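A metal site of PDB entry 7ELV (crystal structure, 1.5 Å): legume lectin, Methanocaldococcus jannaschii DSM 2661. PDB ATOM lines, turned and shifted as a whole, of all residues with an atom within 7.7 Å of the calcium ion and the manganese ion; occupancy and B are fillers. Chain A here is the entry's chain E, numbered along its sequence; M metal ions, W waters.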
ATOM      1  N   ALA A  62     -10.975   3.174 -10.670  1.00  0.00           N
ATOM      2  CA  ALA A  62     -10.100   3.683  -9.615  1.00  0.00           C
ATOM      3  C   ALA A  62      -8.987   4.479 -10.255  1.00  0.00           C
ATOM      4  O   ALA A  62      -8.849   4.392 -11.483  1.00  0.00           O
ATOM      5  CB  ALA A  62      -9.542   2.534  -8.812  1.00  0.00           C
ATOM      6  N   ASP A  63      -8.192   5.223  -9.465  1.00  0.00           N
ATOM      7  CA  ASP A  63      -8.275   5.414  -8.024  1.00  0.00           C
ATOM      8  C   ASP A  63      -8.654   6.854  -7.658  1.00  0.00           C
ATOM      9  O   ASP A  63      -9.090   7.038  -6.511  1.00  0.00           O
ATOM     10  CB  ASP A  63      -6.946   5.103  -7.338  1.00  0.00           C
ATOM     11  CG  ASP A  63      -6.809   3.639  -7.014  1.00  0.00           C
ATOM     12  OD1 ASP A  63      -7.319   3.278  -5.937  1.00  0.00           O
ATOM     13  OD2 ASP A  63      -6.224   2.906  -7.839  1.00  0.00           O
ATOM     14  N   GLY A  64      -8.446   7.835  -8.532  1.00  0.00           N
ATOM     15  CA  GLY A  64      -8.690   9.235  -8.219  1.00  0.00           C
ATOM     16  C   GLY A  64      -7.486  10.124  -8.460  1.00  0.00           C
ATOM     17  O   GLY A  64      -6.447   9.707  -8.989  1.00  0.00           O
ATOM     18  N   GLY A  81      -1.977   3.549  -7.403  1.00  0.00           N
ATOM     19  CA  GLY A  81      -3.174   2.974  -6.771  1.00  0.00           C
ATOM     20  C   GLY A  81      -3.844   3.979  -5.822  1.00  0.00           C
ATOM     21  O   GLY A  81      -4.024   5.188  -6.194  1.00  0.00           O
ATOM     22  N   GLY A  82      -4.166   3.545  -4.604  1.00  0.00           N
ATOM     23  CA  GLY A  82      -4.905   4.374  -3.641  1.00  0.00           C
ATOM     24  C   GLY A  82      -4.059   5.529  -3.129  1.00  0.00           C
ATOM     25  O   GLY A  82      -4.572   6.370  -2.424  1.00  0.00           O
ATOM     26  N   ASP A  83      -2.774   5.588  -3.449  1.00  0.00           N
ATOM     27  CA  ASP A  83      -1.941   6.771  -3.147  1.00  0.00           C
ATOM     28  C   ASP A  83      -2.268   7.939  -4.105  1.00  0.00           C
ATOM     29  O   ASP A  83      -1.842   9.036  -3.813  1.00  0.00           O
ATOM     30  CB  ASP A  83      -0.462   6.431  -3.228  1.00  0.00           C
ATOM     31  CG  ASP A  83       0.130   5.899  -1.929  1.00  0.00           C
ATOM     32  OD1 ASP A  83      -0.577   5.876  -0.910  1.00  0.00           O
ATOM     33  OD2 ASP A  83       1.311   5.607  -1.928  1.00  0.00           O
ATOM     34  N   LEU A  84      -2.961   7.687  -5.207  1.00  0.00           N
ATOM     35  CA  LEU A  84      -3.494   8.735  -6.125  1.00  0.00           C
ATOM     36  C   LEU A  84      -2.385   9.529  -6.811  1.00  0.00           C
ATOM     37  O   LEU A  84      -2.680  10.610  -7.293  1.00  0.00           O
ATOM     38  CB  LEU A  84      -4.384   9.719  -5.330  1.00  0.00           C
ATOM     39  CG  LEU A  84      -5.458   9.109  -4.428  1.00  0.00           C
ATOM     40  CD1 LEU A  84      -6.349  10.195  -3.797  1.00  0.00           C
ATOM     41  CD2 LEU A  84      -6.285   8.134  -5.206  1.00  0.00           C
ATOM     42  N   GLU A  96      -8.174  15.689  -2.537  1.00  0.00           N
ATOM     43  CA  GLU A  96      -8.324  14.471  -3.338  1.00  0.00           C
ATOM     44  C   GLU A  96      -9.752  14.357  -3.837  1.00  0.00           C
ATOM     45  O   GLU A  96     -10.669  14.718  -3.069  1.00  0.00           O
ATOM     46  CB  GLU A  96      -7.914  13.196  -2.576  1.00  0.00           C
ATOM     47  CG  GLU A  96      -8.679  12.924  -1.305  1.00  0.00           C
ATOM     48  CD  GLU A  96      -8.400  11.533  -0.733  1.00  0.00           C
ATOM     49  OE1 GLU A  96      -7.212  11.197  -0.457  1.00  0.00           O
ATOM     50  OE2 GLU A  96      -9.412  10.773  -0.625  1.00  0.00           O
ATOM     51  N   VAL A  97      -9.905  13.771  -5.004  1.00  0.00           N
ATOM     52  CA  VAL A  97     -11.194  13.268  -5.533  1.00  0.00           C
ATOM     53  C   VAL A  97     -10.941  11.784  -5.723  1.00  0.00           C
ATOM     54  O   VAL A  97     -10.234  11.370  -6.650  1.00  0.00           O
ATOM     55  CB  VAL A  97     -11.647  13.970  -6.806  1.00  0.00           C
ATOM     56  CG1 VAL A  97     -12.986  13.384  -7.191  1.00  0.00           C
ATOM     57  CG2 VAL A  97     -11.762  15.474  -6.568  1.00  0.00           C
ATOM     58  N   ASP A  98     -11.462  10.991  -4.788  1.00  0.00           N
ATOM     59  CA  ASP A  98     -11.062   9.595  -4.555  1.00  0.00           C
ATOM     60  C   ASP A  98     -12.189   8.713  -5.064  1.00  0.00           C
ATOM     61  O   ASP A  98     -13.308   8.860  -4.554  1.00  0.00           O
ATOM     62  CB  ASP A  98     -10.745   9.385  -3.088  1.00  0.00           C
ATOM     63  CG  ASP A  98     -10.278   7.979  -2.726  1.00  0.00           C
ATOM     64  OD1 ASP A  98     -10.442   7.087  -3.566  1.00  0.00           O
ATOM     65  OD2 ASP A  98      -9.734   7.835  -1.643  1.00  0.00           O
ATOM     66  N   THR A  99     -11.923   7.793  -5.992  1.00  0.00           N
ATOM     67  CA  THR A  99     -12.981   7.047  -6.710  1.00  0.00           C
ATOM     68  C   THR A  99     -12.916   5.548  -6.362  1.00  0.00           C
ATOM     69  O   THR A  99     -13.605   4.790  -7.039  1.00  0.00           O
ATOM     70  CB  THR A  99     -12.896   7.293  -8.220  1.00  0.00           C
ATOM     71  OG1 THR A  99     -11.613   6.842  -8.635  1.00  0.00           O
ATOM     72  CG2 THR A  99     -13.107   8.754  -8.575  1.00  0.00           C
ATOM     73  N   TRP A 100     -12.182   5.146  -5.336  1.00  0.00           N
ATOM     74  CA  TRP A 100     -12.115   3.719  -4.950  1.00  0.00           C
ATOM     75  C   TRP A 100     -11.991   3.645  -3.450  1.00  0.00           C
ATOM     76  O   TRP A 100     -11.126   4.251  -2.840  1.00  0.00           O
ATOM     77  CB  TRP A 100     -10.952   3.020  -5.654  1.00  0.00           C
ATOM     78  CG  TRP A 100     -10.738   1.624  -5.163  1.00  0.00           C
ATOM     79  CD1 TRP A 100     -10.028   1.213  -4.063  1.00  0.00           C
ATOM     80  CD2 TRP A 100     -11.246   0.461  -5.801  1.00  0.00           C
ATOM     81  NE1 TRP A 100     -10.059  -0.150  -3.990  1.00  0.00           N
ATOM     82  CE2 TRP A 100     -10.798  -0.623  -5.024  1.00  0.00           C
ATOM     83  CE3 TRP A 100     -12.028   0.244  -6.925  1.00  0.00           C
ATOM     84  CZ2 TRP A 100     -11.094  -1.945  -5.382  1.00  0.00           C
ATOM     85  CZ3 TRP A 100     -12.325  -1.057  -7.274  1.00  0.00           C
ATOM     86  CH2 TRP A 100     -11.865  -2.125  -6.508  1.00  0.00           C
ATOM     87  N   LEU A 101     -12.909   2.905  -2.802  1.00  0.00           N
ATOM     88  CA  LEU A 101     -12.902   2.853  -1.330  1.00  0.00           C
ATOM     89  C   LEU A 101     -11.889   1.838  -0.845  1.00  0.00           C
ATOM     90  O   LEU A 101     -12.153   0.609  -0.930  1.00  0.00           O
ATOM     91  CB  LEU A 101     -14.305   2.463  -0.845  1.00  0.00           C
ATOM     92  CG  LEU A 101     -15.363   3.524  -0.910  1.00  0.00           C
ATOM     93  CD1 LEU A 101     -16.713   2.944  -0.519  1.00  0.00           C
ATOM     94  CD2 LEU A 101     -15.046   4.698   0.028  1.00  0.00           C
ATOM     95  N   ASN A 102     -10.800   2.330  -0.293  1.00  0.00           N
ATOM     96  CA  ASN A 102      -9.781   1.523   0.406  1.00  0.00           C
ATOM     97  C   ASN A 102     -10.183   1.318   1.865  1.00  0.00           C
ATOM     98  O   ASN A 102     -10.957   2.105   2.383  1.00  0.00           O
ATOM     99  CB  ASN A 102      -8.402   2.166   0.288  1.00  0.00           C
ATOM    100  CG  ASN A 102      -7.944   2.312  -1.147  1.00  0.00           C
ATOM    101  OD1 ASN A 102      -8.236   3.333  -1.789  1.00  0.00           O
ATOM    102  ND2 ASN A 102      -7.290   1.292  -1.700  1.00  0.00           N
ATOM    103  N   ASP A 103      -9.592   0.354   2.580  1.00  0.00           N
ATOM    104  CA  ASP A 103      -9.981   0.213   4.014  1.00  0.00           C
ATOM    105  C   ASP A 103      -9.659   1.527   4.756  1.00  0.00           C
ATOM    106  O   ASP A 103     -10.465   1.954   5.622  1.00  0.00           O
ATOM    107  CB  ASP A 103      -9.321  -1.013   4.659  1.00  0.00           C
ATOM    108  CG  ASP A 103      -7.872  -1.230   4.262  1.00  0.00           C
ATOM    109  OD1 ASP A 103      -7.248  -0.273   3.714  1.00  0.00           O
ATOM    110  OD2 ASP A 103      -7.368  -2.354   4.516  1.00  0.00           O
ATOM    111  N   PHE A 104      -8.599   2.236   4.350  1.00  0.00           N
ATOM    112  CA  PHE A 104      -8.142   3.460   5.053  1.00  0.00           C
ATOM    113  C   PHE A 104      -9.020   4.683   4.702  1.00  0.00           C
ATOM    114  O   PHE A 104      -8.714   5.762   5.178  1.00  0.00           O
ATOM    115  CB  PHE A 104      -6.653   3.719   4.759  1.00  0.00           C
ATOM    116  CG  PHE A 104      -6.271   3.779   3.295  1.00  0.00           C
ATOM    117  CD1 PHE A 104      -6.665   4.857   2.519  1.00  0.00           C
ATOM    118  CD2 PHE A 104      -5.557   2.754   2.684  1.00  0.00           C
ATOM    119  CE1 PHE A 104      -6.297   4.936   1.182  1.00  0.00           C
ATOM    120  CE2 PHE A 104      -5.214   2.833   1.344  1.00  0.00           C
ATOM    121  CZ  PHE A 104      -5.575   3.938   0.601  1.00  0.00           C
ATOM    122  N   ASP A 105     -10.021   4.497   3.862  1.00  0.00           N
ATOM    123  CA  ASP A 105     -10.868   5.608   3.377  1.00  0.00           C
ATOM    124  C   ASP A 105     -12.019   5.874   4.352  1.00  0.00           C
ATOM    125  O   ASP A 105     -12.692   6.887   4.207  1.00  0.00           O
ATOM    126  CB  ASP A 105     -11.383   5.396   1.965  1.00  0.00           C
ATOM    127  CG  ASP A 105     -10.393   5.791   0.886  1.00  0.00           C
ATOM    128  OD1 ASP A 105      -9.786   6.865   1.103  1.00  0.00           O
ATOM    129  OD2 ASP A 105     -10.325   5.101  -0.142  1.00  0.00           O
ATOM    130  N   ALA A 106     -12.251   5.010   5.337  1.00  0.00           N
ATOM    131  CA  ALA A 106     -13.336   5.270   6.307  1.00  0.00           C
ATOM    132  C   ALA A 106     -13.101   6.652   6.892  1.00  0.00           C
ATOM    133  O   ALA A 106     -11.943   7.018   7.201  1.00  0.00           O
ATOM    134  CB  ALA A 106     -13.310   4.209   7.382  1.00  0.00           C
ATOM    135  N   ALA A 108     -15.490   7.631   4.608  1.00  0.00           N
ATOM    136  CA  ALA A 108     -16.118   7.744   3.294  1.00  0.00           C
ATOM    137  C   ALA A 108     -16.902   6.470   2.951  1.00  0.00           C
ATOM    138  O   ALA A 108     -16.491   5.320   3.342  1.00  0.00           O
ATOM    139  CB  ALA A 108     -15.053   8.021   2.244  1.00  0.00           C
ATOM    140  N   THR A 110     -18.630   6.615  -0.542  1.00  0.00           N
ATOM    141  CA  THR A 110     -18.808   6.683  -2.002  1.00  0.00           C
ATOM    142  C   THR A 110     -17.530   7.308  -2.565  1.00  0.00           C
ATOM    143  O   THR A 110     -16.648   7.637  -1.774  1.00  0.00           O
ATOM    144  CB  THR A 110     -20.035   7.488  -2.421  1.00  0.00           C
ATOM    145  OG1 THR A 110     -19.812   8.882  -2.168  1.00  0.00           O
ATOM    146  CG2 THR A 110     -21.297   7.068  -1.694  1.00  0.00           C
ATOM    147  N   HIS A 112     -15.372  10.372  -3.162  1.00  0.00           N
ATOM    148  CA  HIS A 112     -15.372  11.400  -2.108  1.00  0.00           C
ATOM    149  C   HIS A 112     -14.304  12.446  -2.353  1.00  0.00           C
ATOM    150  O   HIS A 112     -13.344  12.180  -3.099  1.00  0.00           O
ATOM    151  CB  HIS A 112     -15.205  10.805  -0.700  1.00  0.00           C
ATOM    152  CG  HIS A 112     -14.000   9.929  -0.538  1.00  0.00           C
ATOM    153  ND1 HIS A 112     -14.015   8.593  -0.902  1.00  0.00           N
ATOM    154  CD2 HIS A 112     -12.758  10.185  -0.030  1.00  0.00           C
ATOM    155  CE1 HIS A 112     -12.832   8.089  -0.644  1.00  0.00           C
ATOM    156  NE2 HIS A 112     -12.062   8.996  -0.075  1.00  0.00           N
ATOM    157  N   ILE A 113     -14.522  13.600  -1.771  1.00  0.00           N
ATOM    158  CA  ILE A 113     -13.518  14.681  -1.752  1.00  0.00           C
ATOM    159  C   ILE A 113     -13.009  14.833  -0.338  1.00  0.00           C
ATOM    160  O   ILE A 113     -13.820  14.760   0.631  1.00  0.00           O
ATOM    161  CB  ILE A 113     -14.137  15.910  -2.467  1.00  0.00           C
ATOM    162  CG1 ILE A 113     -13.095  16.982  -2.782  1.00  0.00           C
ATOM    163  CG2 ILE A 113     -15.316  16.480  -1.726  1.00  0.00           C
ATOM    164  CD1 ILE A 113     -13.485  17.923  -3.918  1.00  0.00           C
ATOM    165  N   ALA A 114     -11.715  15.046  -0.138  1.00  0.00           N
ATOM    166  CA  ALA A 114     -11.107  15.117   1.185  1.00  0.00           C
ATOM    167  C   ALA A 114      -9.844  15.983   1.151  1.00  0.00           C
ATOM    168  O   ALA A 114      -9.227  16.124   0.064  1.00  0.00           O
ATOM    169  CB  ALA A 114     -10.779  13.740   1.722  1.00  0.00           C
ATOM    170  N   ASP A 116      -6.040  16.048   2.498  1.00  0.00           N
ATOM    171  CA  ASP A 116      -4.928  15.224   2.997  1.00  0.00           C
ATOM    172  C   ASP A 116      -3.745  16.112   3.340  1.00  0.00           C
ATOM    173  O   ASP A 116      -3.574  17.181   2.763  1.00  0.00           O
ATOM    174  CB  ASP A 116      -4.495  14.258   1.911  1.00  0.00           C
ATOM    175  CG  ASP A 116      -5.531  13.285   1.425  1.00  0.00           C
ATOM    176  OD1 ASP A 116      -6.446  12.956   2.220  1.00  0.00           O
ATOM    177  OD2 ASP A 116      -5.468  12.897   0.256  1.00  0.00           O
ATOM    178  N   ILE A 121      -2.915   9.527   3.209  1.00  0.00           N
ATOM    179  CA  ILE A 121      -4.199   9.339   2.483  1.00  0.00           C
ATOM    180  C   ILE A 121      -5.225   8.610   3.390  1.00  0.00           C
ATOM    181  O   ILE A 121      -6.329   8.336   2.904  1.00  0.00           O
ATOM    182  CB  ILE A 121      -3.994   8.656   1.114  1.00  0.00           C
ATOM    183  CG1 ILE A 121      -3.097   7.417   1.123  1.00  0.00           C
ATOM    184  CG2 ILE A 121      -3.420   9.643   0.098  1.00  0.00           C
ATOM    185  CD1 ILE A 121      -3.503   6.359   2.062  1.00  0.00           C
ATOM    186  N   ASN A 122      -4.890   8.367   4.668  1.00  0.00           N
ATOM    187  CA  ASN A 122      -5.773   7.672   5.649  1.00  0.00           C
ATOM    188  C   ASN A 122      -6.634   8.711   6.387  1.00  0.00           C
ATOM    189  O   ASN A 122      -6.074   9.528   7.201  1.00  0.00           O
ATOM    190  CB  ASN A 122      -4.906   6.887   6.627  1.00  0.00           C
ATOM    191  CG  ASN A 122      -5.659   6.107   7.686  1.00  0.00           C
ATOM    192  OD1 ASN A 122      -6.583   6.615   8.298  1.00  0.00           O
ATOM    193  ND2 ASN A 122      -5.235   4.866   7.913  1.00  0.00           N
ATOM    194  N   HIS A 123      -7.936   8.696   6.164  1.00  0.00           N
ATOM    195  CA  HIS A 123      -8.758   9.856   6.641  1.00  0.00           C
ATOM    196  C   HIS A 123      -8.856   9.908   8.180  1.00  0.00           C
ATOM    197  O   HIS A 123      -8.835  11.018   8.737  1.00  0.00           O
ATOM    198  CB  HIS A 123     -10.086   9.884   5.912  1.00  0.00           C
ATOM    199  CG  HIS A 123      -9.859   9.988   4.432  1.00  0.00           C
ATOM    200  ND1 HIS A 123      -8.998  10.958   3.894  1.00  0.00           N
ATOM    201  CD2 HIS A 123     -10.342   9.295   3.411  1.00  0.00           C
ATOM    202  CE1 HIS A 123      -8.995  10.756   2.580  1.00  0.00           C
ATOM    203  NE2 HIS A 123      -9.795   9.784   2.257  1.00  0.00           N
ATOM    204  N   PRO A 135     -14.010  13.117   5.148  1.00  0.00           N
ATOM    205  CA  PRO A 135     -14.267  13.111   3.722  1.00  0.00           C
ATOM    206  C   PRO A 135     -15.729  13.417   3.444  1.00  0.00           C
ATOM    207  O   PRO A 135     -16.629  13.066   4.225  1.00  0.00           O
ATOM    208  CB  PRO A 135     -13.904  11.712   3.231  1.00  0.00           C
ATOM    209  CG  PRO A 135     -13.581  10.930   4.475  1.00  0.00           C
ATOM    210  CD  PRO A 135     -13.553  11.832   5.674  1.00  0.00           C
HETATM  211 CA    CA M   1      -9.200   5.445  -2.207  1.00  0.00          CA
HETATM  212 MN    MN M   2      -9.776   8.852   0.248  1.00  0.00          MN
HETATM  213  O   HOH W   1      -7.157   6.560  -1.580  1.00  0.00           O
HETATM  214  O   HOH W   2      -7.471   8.667   0.312  1.00  0.00           O
HETATM  215  O   HOH W   3      -8.365   5.225  -4.430  1.00  0.00           O
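Of the 28 residues printed, 4 come within 4 Å of the calcium ion.
The nearest printed residue that does not touch the calcium ion is Phe 104 (4.5 Å).
The manganese ion is bound by OE2 of Glu 96, at 2.1 Å.
The manganese ion is bound by OD2 of Asp 98.
The side-chain carboxylate (OD1) of Asp 105 is bound to the manganese ion (2.2 Å).
The manganese ion is bound by NE2 of His 123, at 2.2 Å.
Water W2 is bound to the manganese ion.
The manganese ion is bound by NE2 of His 112, at 2.3 Å.
Water W2 lies within hydrogen-bond range of the side-chain carboxylate (OE1) of Glu 96 (2.7 Å) and the backbone carbonyl oxygen (O) of Ile 121 (2.9 Å).
O of Trp 100 binds the calcium ion, at 2.4 Å.
OD1 of Asn 102 is bound to the calcium ion, at 2.4 Å.
OD2 of Asp 105 binds the calcium ion (2.4 Å).
The calcium ion is bound by water W3.
Water W1 is bound to the calcium ion, at 2.4 Å.
OD1 of Asp 98 is bound to the calcium ion.
OD2 of Asp 98 is bound to the calcium ion, at 2.5 Å.
The calcium ion has seven donor atoms within binding distance.
The backbone NH (N) of Glu 96 is in hydrogen-bond range of the backbone carbonyl oxygen (O) of Ala 114.
OE1 of Glu 96 sits close to OD2 of Asp 116.
N of His 123 lies within hydrogen-bond range of O of Phe 104, at 3.2 Å.
A ring nitrogen (ND1) of His 112 sits at hydrogen-bond distance from the backbone carbonyl oxygen of Thr 110, at 2.9 Å.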
